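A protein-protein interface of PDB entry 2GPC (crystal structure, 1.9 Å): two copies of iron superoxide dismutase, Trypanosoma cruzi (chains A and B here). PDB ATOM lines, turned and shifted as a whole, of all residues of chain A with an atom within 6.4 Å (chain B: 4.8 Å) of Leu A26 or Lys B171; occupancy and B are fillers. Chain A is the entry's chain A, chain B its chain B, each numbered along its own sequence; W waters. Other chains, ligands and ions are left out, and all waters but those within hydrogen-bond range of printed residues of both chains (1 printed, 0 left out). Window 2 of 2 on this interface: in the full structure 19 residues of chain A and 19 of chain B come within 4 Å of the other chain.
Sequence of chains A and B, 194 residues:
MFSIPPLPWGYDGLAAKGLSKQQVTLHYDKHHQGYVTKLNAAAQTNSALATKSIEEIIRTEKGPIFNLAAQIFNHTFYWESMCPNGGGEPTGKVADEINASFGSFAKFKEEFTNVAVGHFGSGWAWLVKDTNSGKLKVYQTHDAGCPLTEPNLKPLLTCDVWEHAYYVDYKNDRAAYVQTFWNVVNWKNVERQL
Position printed for both chains: 168.
Water W1 lies within hydrogen-bond range of O of His A164, OH of Tyr B167, N of His A27 and NE2 of Gln A23.
Printed residues of chain A that touch a printed residue of chain B: Leu A26, Lys A30, His A31, His A164 and Val A168.
Hydrophobic or aromatic side chains of chain A within 4 Å of the printed part of chain B: Leu A26, His A31, His A164 and Val A168.
Along chain B the printed residues that touch a printed residue of chain A span positions 167 to 172.
Among the printed residues, no Asp or Glu carboxylate lies within 4 Å of a Lys or Arg side-chain nitrogen of the other chain.
CD of Lys B171 touches CD1 of Leu A26, at 3.8 Å.
Lys A30 touches Asn B172 (CG to ND2, 3.4 Å).
NE2 of His A31 touches CB of Asn B172, 3.7 Å away.
His A164 touches Tyr B167.
Tyr B167 touches Val A168.
NE2 of Gln A23 lies within hydrogen-bond range of O of His A164.
The backbone NH of Val A168 lies within hydrogen-bond range of the side-chain amide oxygen of Gln A23 (3.0 Å).
The backbone carbonyl oxygen (O) of Leu A26 is in hydrogen-bond range of the backbone NH (N) of His A31.
OH of Tyr B167 lies within hydrogen-bond range of NE2 of His A31 (2.7 Å).
Of chain B, only Lys B171 (3.8 Å) comes within 4 Å of Leu A26.
His A27 touches none of the printed residues of chain B.
Of the printed residues of chain B, Lys A30 touches Asn B172.
Of the printed residues of chain B, His A31 touches Tyr B167 and Asn B172.
Printed residues of chain B within 4 Å of His A164: Tyr B167 (3.7 Å).
Of the printed residues of chain A, Tyr B167 touches His A31, His A164 and Val A168.
Lys B171 touches just one residue of chain A: Leu A26 (3.8 Å).
Of the printed residues of chain A, Asn B172 touches Lys A30 and His A31.
The nearest residue of chain A that does not touch Lys B171 is Val A168 (4.5 Å).
The nearest printed residue of chain B that does not touch His A164 is Asn B172 (6.6 Å).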
ATOM      1  N   TYR A  11       9.030  -5.738  31.748  1.00  0.00           N
ATOM      2  CA  TYR A  11       8.906  -7.155  32.097  1.00  0.00           C
ATOM      3  C   TYR A  11       7.696  -7.481  32.996  1.00  0.00           C
ATOM      4  O   TYR A  11       7.038  -8.510  32.798  1.00  0.00           O
ATOM      5  CB  TYR A  11      10.207  -7.659  32.752  1.00  0.00           C
ATOM      6  CG  TYR A  11      11.404  -7.754  31.824  1.00  0.00           C
ATOM      7  CD1 TYR A  11      12.363  -6.751  31.783  1.00  0.00           C
ATOM      8  CD2 TYR A  11      11.579  -8.856  30.994  1.00  0.00           C
ATOM      9  CE1 TYR A  11      13.471  -6.849  30.941  1.00  0.00           C
ATOM     10  CE2 TYR A  11      12.661  -8.957  30.147  1.00  0.00           C
ATOM     11  CZ  TYR A  11      13.616  -7.959  30.129  1.00  0.00           C
ATOM     12  OH  TYR A  11      14.704  -8.062  29.288  1.00  0.00           O
ATOM     13  N   LYS A  21       5.802 -11.412  35.491  1.00  0.00           N
ATOM     14  CA  LYS A  21       7.175 -11.025  35.183  1.00  0.00           C
ATOM     15  C   LYS A  21       7.999 -12.216  34.703  1.00  0.00           C
ATOM     16  O   LYS A  21       8.747 -12.102  33.730  1.00  0.00           O
ATOM     17  CB  LYS A  21       7.855 -10.367  36.385  1.00  0.00           C
ATOM     18  CG  LYS A  21       9.178  -9.700  36.040  1.00  0.00           C
ATOM     19  CD  LYS A  21       9.766  -8.952  37.234  1.00  0.00           C
ATOM     20  CE  LYS A  21      10.950  -8.093  36.823  1.00  0.00           C
ATOM     21  NZ  LYS A  21      11.730  -7.614  37.997  1.00  0.00           N
ATOM     22  N   GLN A  22       7.855 -13.360  35.370  1.00  0.00           N
ATOM     23  CA  GLN A  22       8.649 -14.536  35.034  1.00  0.00           C
ATOM     24  C   GLN A  22       8.258 -15.119  33.665  1.00  0.00           C
ATOM     25  O   GLN A  22       9.135 -15.419  32.866  1.00  0.00           O
ATOM     26  CB  GLN A  22       8.580 -15.578  36.166  1.00  0.00           C
ATOM     27  CG  GLN A  22       9.246 -16.913  35.879  1.00  0.00           C
ATOM     28  CD  GLN A  22      10.769 -16.848  35.799  1.00  0.00           C
ATOM     29  OE1 GLN A  22      11.378 -15.776  35.919  1.00  0.00           O
ATOM     30  NE2 GLN A  22      11.384 -18.006  35.621  1.00  0.00           N
ATOM     31  N   GLN A  23       6.958 -15.237  33.386  1.00  0.00           N
ATOM     32  CA  GLN A  23       6.477 -15.726  32.086  1.00  0.00           C
ATOM     33  C   GLN A  23       6.962 -14.828  30.952  1.00  0.00           C
ATOM     34  O   GLN A  23       7.404 -15.306  29.903  1.00  0.00           O
ATOM     35  CB  GLN A  23       4.943 -15.796  32.076  1.00  0.00           C
ATOM     36  CG  GLN A  23       4.296 -16.147  30.750  1.00  0.00           C
ATOM     37  CD  GLN A  23       4.579 -17.566  30.312  1.00  0.00           C
ATOM     38  OE1 GLN A  23       3.861 -18.483  30.688  1.00  0.00           O
ATOM     39  NE2 GLN A  23       5.628 -17.750  29.517  1.00  0.00           N
ATOM     40  N   VAL A  24       6.852 -13.525  31.162  1.00  0.00           N
ATOM     41  CA  VAL A  24       7.237 -12.552  30.157  1.00  0.00           C
ATOM     42  C   VAL A  24       8.752 -12.540  29.982  1.00  0.00           C
ATOM     43  O   VAL A  24       9.238 -12.488  28.862  1.00  0.00           O
ATOM     44  CB  VAL A  24       6.712 -11.143  30.511  1.00  0.00           C
ATOM     45  CG1 VAL A  24       7.385 -10.067  29.654  1.00  0.00           C
ATOM     46  CG2 VAL A  24       5.197 -11.100  30.351  1.00  0.00           C
ATOM     47  N   THR A  25       9.486 -12.619  31.086  1.00  0.00           N
ATOM     48  CA  THR A  25      10.955 -12.581  31.056  1.00  0.00           C
ATOM     49  C   THR A  25      11.559 -13.743  30.282  1.00  0.00           C
ATOM     50  O   THR A  25      12.436 -13.545  29.446  1.00  0.00           O
ATOM     51  CB  THR A  25      11.529 -12.544  32.491  1.00  0.00           C
ATOM     52  OG1 THR A  25      11.175 -11.297  33.103  1.00  0.00           O
ATOM     53  CG2 THR A  25      13.049 -12.531  32.480  1.00  0.00           C
ATOM     54  N   LEU A  26      11.109 -14.957  30.574  1.00  0.00           N
ATOM     55  CA  LEU A  26      11.559 -16.128  29.831  1.00  0.00           C
ATOM     56  C   LEU A  26      11.203 -15.981  28.360  1.00  0.00           C
ATOM     57  O   LEU A  26      12.035 -16.205  27.485  1.00  0.00           O
ATOM     58  CB  LEU A  26      10.943 -17.413  30.396  1.00  0.00           C
ATOM     59  CG  LEU A  26      11.485 -17.882  31.744  1.00  0.00           C
ATOM     60  CD1 LEU A  26      10.525 -18.893  32.318  1.00  0.00           C
ATOM     61  CD2 LEU A  26      12.891 -18.467  31.641  1.00  0.00           C
ATOM     62  N   HIS A  27       9.962 -15.596  28.088  1.00  0.00           N
ATOM     63  CA  HIS A  27       9.490 -15.484  26.710  1.00  0.00           C
ATOM     64  C   HIS A  27      10.322 -14.448  25.914  1.00  0.00           C
ATOM     65  O   HIS A  27      10.729 -14.721  24.787  1.00  0.00           O
ATOM     66  CB  HIS A  27       7.981 -15.185  26.705  1.00  0.00           C
ATOM     67  CG  HIS A  27       7.292 -15.464  25.406  1.00  0.00           C
ATOM     68  ND1 HIS A  27       5.963 -15.166  25.207  1.00  0.00           N
ATOM     69  CD2 HIS A  27       7.733 -16.019  24.248  1.00  0.00           C
ATOM     70  CE1 HIS A  27       5.612 -15.519  23.979  1.00  0.00           C
ATOM     71  NE2 HIS A  27       6.668 -16.038  23.376  1.00  0.00           N
ATOM     72  N   TYR A  28      10.646 -13.311  26.526  1.00  0.00           N
ATOM     73  CA  TYR A  28      11.388 -12.247  25.846  1.00  0.00           C
ATOM     74  C   TYR A  28      12.896 -12.503  25.831  1.00  0.00           C
ATOM     75  O   TYR A  28      13.526 -12.459  24.777  1.00  0.00           O
ATOM     76  CB  TYR A  28      11.094 -10.878  26.500  1.00  0.00           C
ATOM     77  CG  TYR A  28      11.730  -9.707  25.785  1.00  0.00           C
ATOM     78  CD1 TYR A  28      11.081  -9.084  24.718  1.00  0.00           C
ATOM     79  CD2 TYR A  28      12.984  -9.230  26.158  1.00  0.00           C
ATOM     80  CE1 TYR A  28      11.657  -8.017  24.044  1.00  0.00           C
ATOM     81  CE2 TYR A  28      13.577  -8.149  25.490  1.00  0.00           C
ATOM     82  CZ  TYR A  28      12.906  -7.550  24.429  1.00  0.00           C
ATOM     83  OH  TYR A  28      13.470  -6.484  23.748  1.00  0.00           O
ATOM     84  N   ASP A  29      13.480 -12.754  26.998  1.00  0.00           N
ATOM     85  CA  ASP A  29      14.938 -12.891  27.117  1.00  0.00           C
ATOM     86  C   ASP A  29      15.464 -14.198  26.519  1.00  0.00           C
ATOM     87  O   ASP A  29      16.553 -14.214  25.941  1.00  0.00           O
ATOM     88  CB  ASP A  29      15.411 -12.817  28.581  1.00  0.00           C
ATOM     89  CG  ASP A  29      15.389 -11.403  29.162  1.00  0.00           C
ATOM     90  OD1 ASP A  29      15.228 -10.383  28.428  1.00  0.00           O
ATOM     91  OD2 ASP A  29      15.553 -11.236  30.382  1.00  0.00           O
ATOM     92  N   LYS A  30      14.728 -15.294  26.692  1.00  0.00           N
ATOM     93  CA  LYS A  30      15.185 -16.585  26.176  1.00  0.00           C
ATOM     94  C   LYS A  30      14.705 -16.834  24.743  1.00  0.00           C
ATOM     95  O   LYS A  30      15.529 -17.038  23.834  1.00  0.00           O
ATOM     96  CB  LYS A  30      14.770 -17.737  27.094  1.00  0.00           C
ATOM     97  CG  LYS A  30      15.278 -17.642  28.541  1.00  0.00           C
ATOM     98  CD  LYS A  30      16.801 -17.474  28.620  1.00  0.00           C
ATOM     99  CE  LYS A  30      17.297 -17.543  30.058  1.00  0.00           C
ATOM    100  NZ  LYS A  30      18.770 -17.303  30.111  1.00  0.00           N
ATOM    101  N   HIS A  31      13.392 -16.813  24.523  1.00  0.00           N
ATOM    102  CA  HIS A  31      12.858 -17.142  23.205  1.00  0.00           C
ATOM    103  C   HIS A  31      13.079 -16.016  22.203  1.00  0.00           C
ATOM    104  O   HIS A  31      13.726 -16.229  21.192  1.00  0.00           O
ATOM    105  CB  HIS A  31      11.374 -17.569  23.281  1.00  0.00           C
ATOM    106  CG  HIS A  31      11.167 -18.831  24.052  1.00  0.00           C
ATOM    107  ND1 HIS A  31      11.378 -20.076  23.501  1.00  0.00           N
ATOM    108  CD2 HIS A  31      10.821 -19.045  25.343  1.00  0.00           C
ATOM    109  CE1 HIS A  31      11.170 -21.002  24.420  1.00  0.00           C
ATOM    110  NE2 HIS A  31      10.833 -20.405  25.548  1.00  0.00           N
ATOM    111  N   HIS A  32      12.590 -14.816  22.492  1.00  0.00           N
ATOM    112  CA  HIS A  32      12.628 -13.737  21.507  1.00  0.00           C
ATOM    113  C   HIS A  32      14.066 -13.303  21.216  1.00  0.00           C
ATOM    114  O   HIS A  32      14.478 -13.245  20.054  1.00  0.00           O
ATOM    115  CB  HIS A  32      11.776 -12.557  21.964  1.00  0.00           C
ATOM    116  CG  HIS A  32      11.384 -11.623  20.859  1.00  0.00           C
ATOM    117  ND1 HIS A  32      10.696 -10.452  21.091  1.00  0.00           N
ATOM    118  CD2 HIS A  32      11.571 -11.688  19.517  1.00  0.00           C
ATOM    119  CE1 HIS A  32      10.484  -9.830  19.944  1.00  0.00           C
ATOM    120  NE2 HIS A  32      11.005 -10.559  18.972  1.00  0.00           N
ATOM    121  N   HIS A 164       5.251 -22.289  25.085  1.00  0.00           N
ATOM    122  CA  HIS A 164       6.159 -21.445  25.863  1.00  0.00           C
ATOM    123  C   HIS A 164       5.578 -20.061  26.190  1.00  0.00           C
ATOM    124  O   HIS A 164       6.018 -19.408  27.121  1.00  0.00           O
ATOM    125  CB  HIS A 164       7.534 -21.304  25.184  1.00  0.00           C
ATOM    126  CG  HIS A 164       7.532 -20.485  23.922  1.00  0.00           C
ATOM    127  ND1 HIS A 164       8.046 -20.960  22.734  1.00  0.00           N
ATOM    128  CD2 HIS A 164       7.128 -19.216  23.672  1.00  0.00           C
ATOM    129  CE1 HIS A 164       7.947 -20.022  21.805  1.00  0.00           C
ATOM    130  NE2 HIS A 164       7.398 -18.954  22.351  1.00  0.00           N
ATOM    131  N   VAL A 168       4.285 -21.303  31.706  1.00  0.00           N
ATOM    132  CA  VAL A 168       4.776 -20.872  33.007  1.00  0.00           C
ATOM    133  C   VAL A 168       3.621 -20.476  33.923  1.00  0.00           C
ATOM    134  O   VAL A 168       3.568 -20.896  35.087  1.00  0.00           O
ATOM    135  CB  VAL A 168       5.793 -19.713  32.852  1.00  0.00           C
ATOM    136  CG1 VAL A 168       6.288 -19.226  34.203  1.00  0.00           C
ATOM    137  CG2 VAL A 168       6.940 -20.144  31.948  1.00  0.00           C
ATOM    138  N   TYR B 166       8.838 -30.644  28.609  1.00  0.00           N
ATOM    139  CA  TYR B 166      10.015 -30.230  29.357  1.00  0.00           C
ATOM    140  C   TYR B 166       9.968 -28.840  29.991  1.00  0.00           C
ATOM    141  O   TYR B 166      10.879 -28.486  30.753  1.00  0.00           O
ATOM    142  CB  TYR B 166      11.246 -30.327  28.450  1.00  0.00           C
ATOM    143  CG  TYR B 166      11.258 -29.451  27.198  1.00  0.00           C
ATOM    144  CD1 TYR B 166      11.705 -28.134  27.239  1.00  0.00           C
ATOM    145  CD2 TYR B 166      10.860 -29.958  25.964  1.00  0.00           C
ATOM    146  CE1 TYR B 166      11.740 -27.346  26.084  1.00  0.00           C
ATOM    147  CE2 TYR B 166      10.895 -29.179  24.814  1.00  0.00           C
ATOM    148  CZ  TYR B 166      11.341 -27.874  24.875  1.00  0.00           C
ATOM    149  OH  TYR B 166      11.372 -27.103  23.714  1.00  0.00           O
ATOM    150  N   TYR B 167       8.924 -28.064  29.717  1.00  0.00           N
ATOM    151  CA  TYR B 167       8.922 -26.654  30.122  1.00  0.00           C
ATOM    152  C   TYR B 167       8.839 -26.456  31.635  1.00  0.00           C
ATOM    153  O   TYR B 167       9.389 -25.493  32.147  1.00  0.00           O
ATOM    154  CB  TYR B 167       7.853 -25.813  29.397  1.00  0.00           C
ATOM    155  CG  TYR B 167       8.398 -24.438  29.044  1.00  0.00           C
ATOM    156  CD1 TYR B 167       9.152 -24.251  27.893  1.00  0.00           C
ATOM    157  CD2 TYR B 167       8.214 -23.350  29.887  1.00  0.00           C
ATOM    158  CE1 TYR B 167       9.694 -23.021  27.576  1.00  0.00           C
ATOM    159  CE2 TYR B 167       8.758 -22.101  29.576  1.00  0.00           C
ATOM    160  CZ  TYR B 167       9.496 -21.947  28.407  1.00  0.00           C
ATOM    161  OH  TYR B 167      10.038 -20.732  28.060  1.00  0.00           O
ATOM    162  N   VAL B 168       8.198 -27.370  32.364  1.00  0.00           N
ATOM    163  CA  VAL B 168       8.132 -27.234  33.831  1.00  0.00           C
ATOM    164  C   VAL B 168       9.510 -27.339  34.488  1.00  0.00           C
ATOM    165  O   VAL B 168       9.854 -26.524  35.335  1.00  0.00           O
ATOM    166  CB  VAL B 168       7.186 -28.253  34.483  1.00  0.00           C
ATOM    167  CG1 VAL B 168       7.111 -28.008  36.014  1.00  0.00           C
ATOM    168  CG2 VAL B 168       5.802 -28.173  33.832  1.00  0.00           C
ATOM    169  N   ASP B 169      10.287 -28.348  34.087  1.00  0.00           N
ATOM    170  CA  ASP B 169      11.597 -28.618  34.679  1.00  0.00           C
ATOM    171  C   ASP B 169      12.766 -27.877  34.013  1.00  0.00           C
ATOM    172  O   ASP B 169      13.757 -27.589  34.676  1.00  0.00           O
ATOM    173  CB  ASP B 169      11.905 -30.109  34.569  1.00  0.00           C
ATOM    174  CG  ASP B 169      11.115 -30.953  35.529  1.00  0.00           C
ATOM    175  OD1 ASP B 169      10.241 -30.438  36.270  1.00  0.00           O
ATOM    176  OD2 ASP B 169      11.301 -32.192  35.587  1.00  0.00           O
ATOM    177  N   TYR B 170      12.661 -27.629  32.705  1.00  0.00           N
ATOM    178  CA  TYR B 170      13.775 -27.112  31.902  1.00  0.00           C
ATOM    179  C   TYR B 170      13.521 -25.748  31.252  1.00  0.00           C
ATOM    180  O   TYR B 170      14.455 -25.119  30.766  1.00  0.00           O
ATOM    181  CB  TYR B 170      14.213 -28.165  30.862  1.00  0.00           C
ATOM    182  CG  TYR B 170      14.724 -29.394  31.561  1.00  0.00           C
ATOM    183  CD1 TYR B 170      16.033 -29.453  32.025  1.00  0.00           C
ATOM    184  CD2 TYR B 170      13.876 -30.465  31.840  1.00  0.00           C
ATOM    185  CE1 TYR B 170      16.499 -30.559  32.720  1.00  0.00           C
ATOM    186  CE2 TYR B 170      14.336 -31.580  32.522  1.00  0.00           C
ATOM    187  CZ  TYR B 170      15.645 -31.616  32.966  1.00  0.00           C
ATOM    188  OH  TYR B 170      16.097 -32.714  33.662  1.00  0.00           O
ATOM    189  N   LYS B 171      12.276 -25.290  31.278  1.00  0.00           N
ATOM    190  CA  LYS B 171      11.865 -24.086  30.569  1.00  0.00           C
ATOM    191  C   LYS B 171      12.365 -24.160  29.104  1.00  0.00           C
ATOM    192  O   LYS B 171      12.108 -25.146  28.420  1.00  0.00           O
ATOM    193  CB  LYS B 171      12.338 -22.828  31.333  1.00  0.00           C
ATOM    194  CG  LYS B 171      12.116 -22.861  32.848  1.00  0.00           C
ATOM    195  CD  LYS B 171      10.672 -22.591  33.260  1.00  0.00           C
ATOM    196  CE  LYS B 171      10.431 -22.866  34.761  1.00  0.00           C
ATOM    197  NZ  LYS B 171       8.988 -22.630  35.187  1.00  0.00           N
ATOM    198  N   ASN B 172      13.097 -23.147  28.638  1.00  0.00           N
ATOM    199  CA  ASN B 172      13.580 -23.064  27.252  1.00  0.00           C
ATOM    200  C   ASN B 172      14.732 -24.009  26.906  1.00  0.00           C
ATOM    201  O   ASN B 172      15.112 -24.130  25.740  1.00  0.00           O
ATOM    202  CB  ASN B 172      14.043 -21.631  26.959  1.00  0.00           C
ATOM    203  CG  ASN B 172      15.260 -21.231  27.784  1.00  0.00           C
ATOM    204  OD1 ASN B 172      16.374 -21.121  27.260  1.00  0.00           O
ATOM    205  ND2 ASN B 172      15.055 -21.028  29.079  1.00  0.00           N
ATOM    206  N   ASP B 173      15.311 -24.647  27.919  1.00  0.00           N
ATOM    207  CA  ASP B 173      16.533 -25.422  27.742  1.00  0.00           C
ATOM    208  C   ASP B 173      16.212 -26.836  27.290  1.00  0.00           C
ATOM    209  O   ASP B 173      16.287 -27.767  28.069  1.00  0.00           O
ATOM    210  CB  ASP B 173      17.335 -25.466  29.054  1.00  0.00           C
ATOM    211  CG  ASP B 173      18.805 -25.786  28.837  1.00  0.00           C
ATOM    212  OD1 ASP B 173      19.191 -26.254  27.740  1.00  0.00           O
ATOM    213  OD2 ASP B 173      19.652 -25.581  29.718  1.00  0.00           O
HETATM  214  O   HOH W   1       8.452 -18.351  27.941  1.00  0.00           O
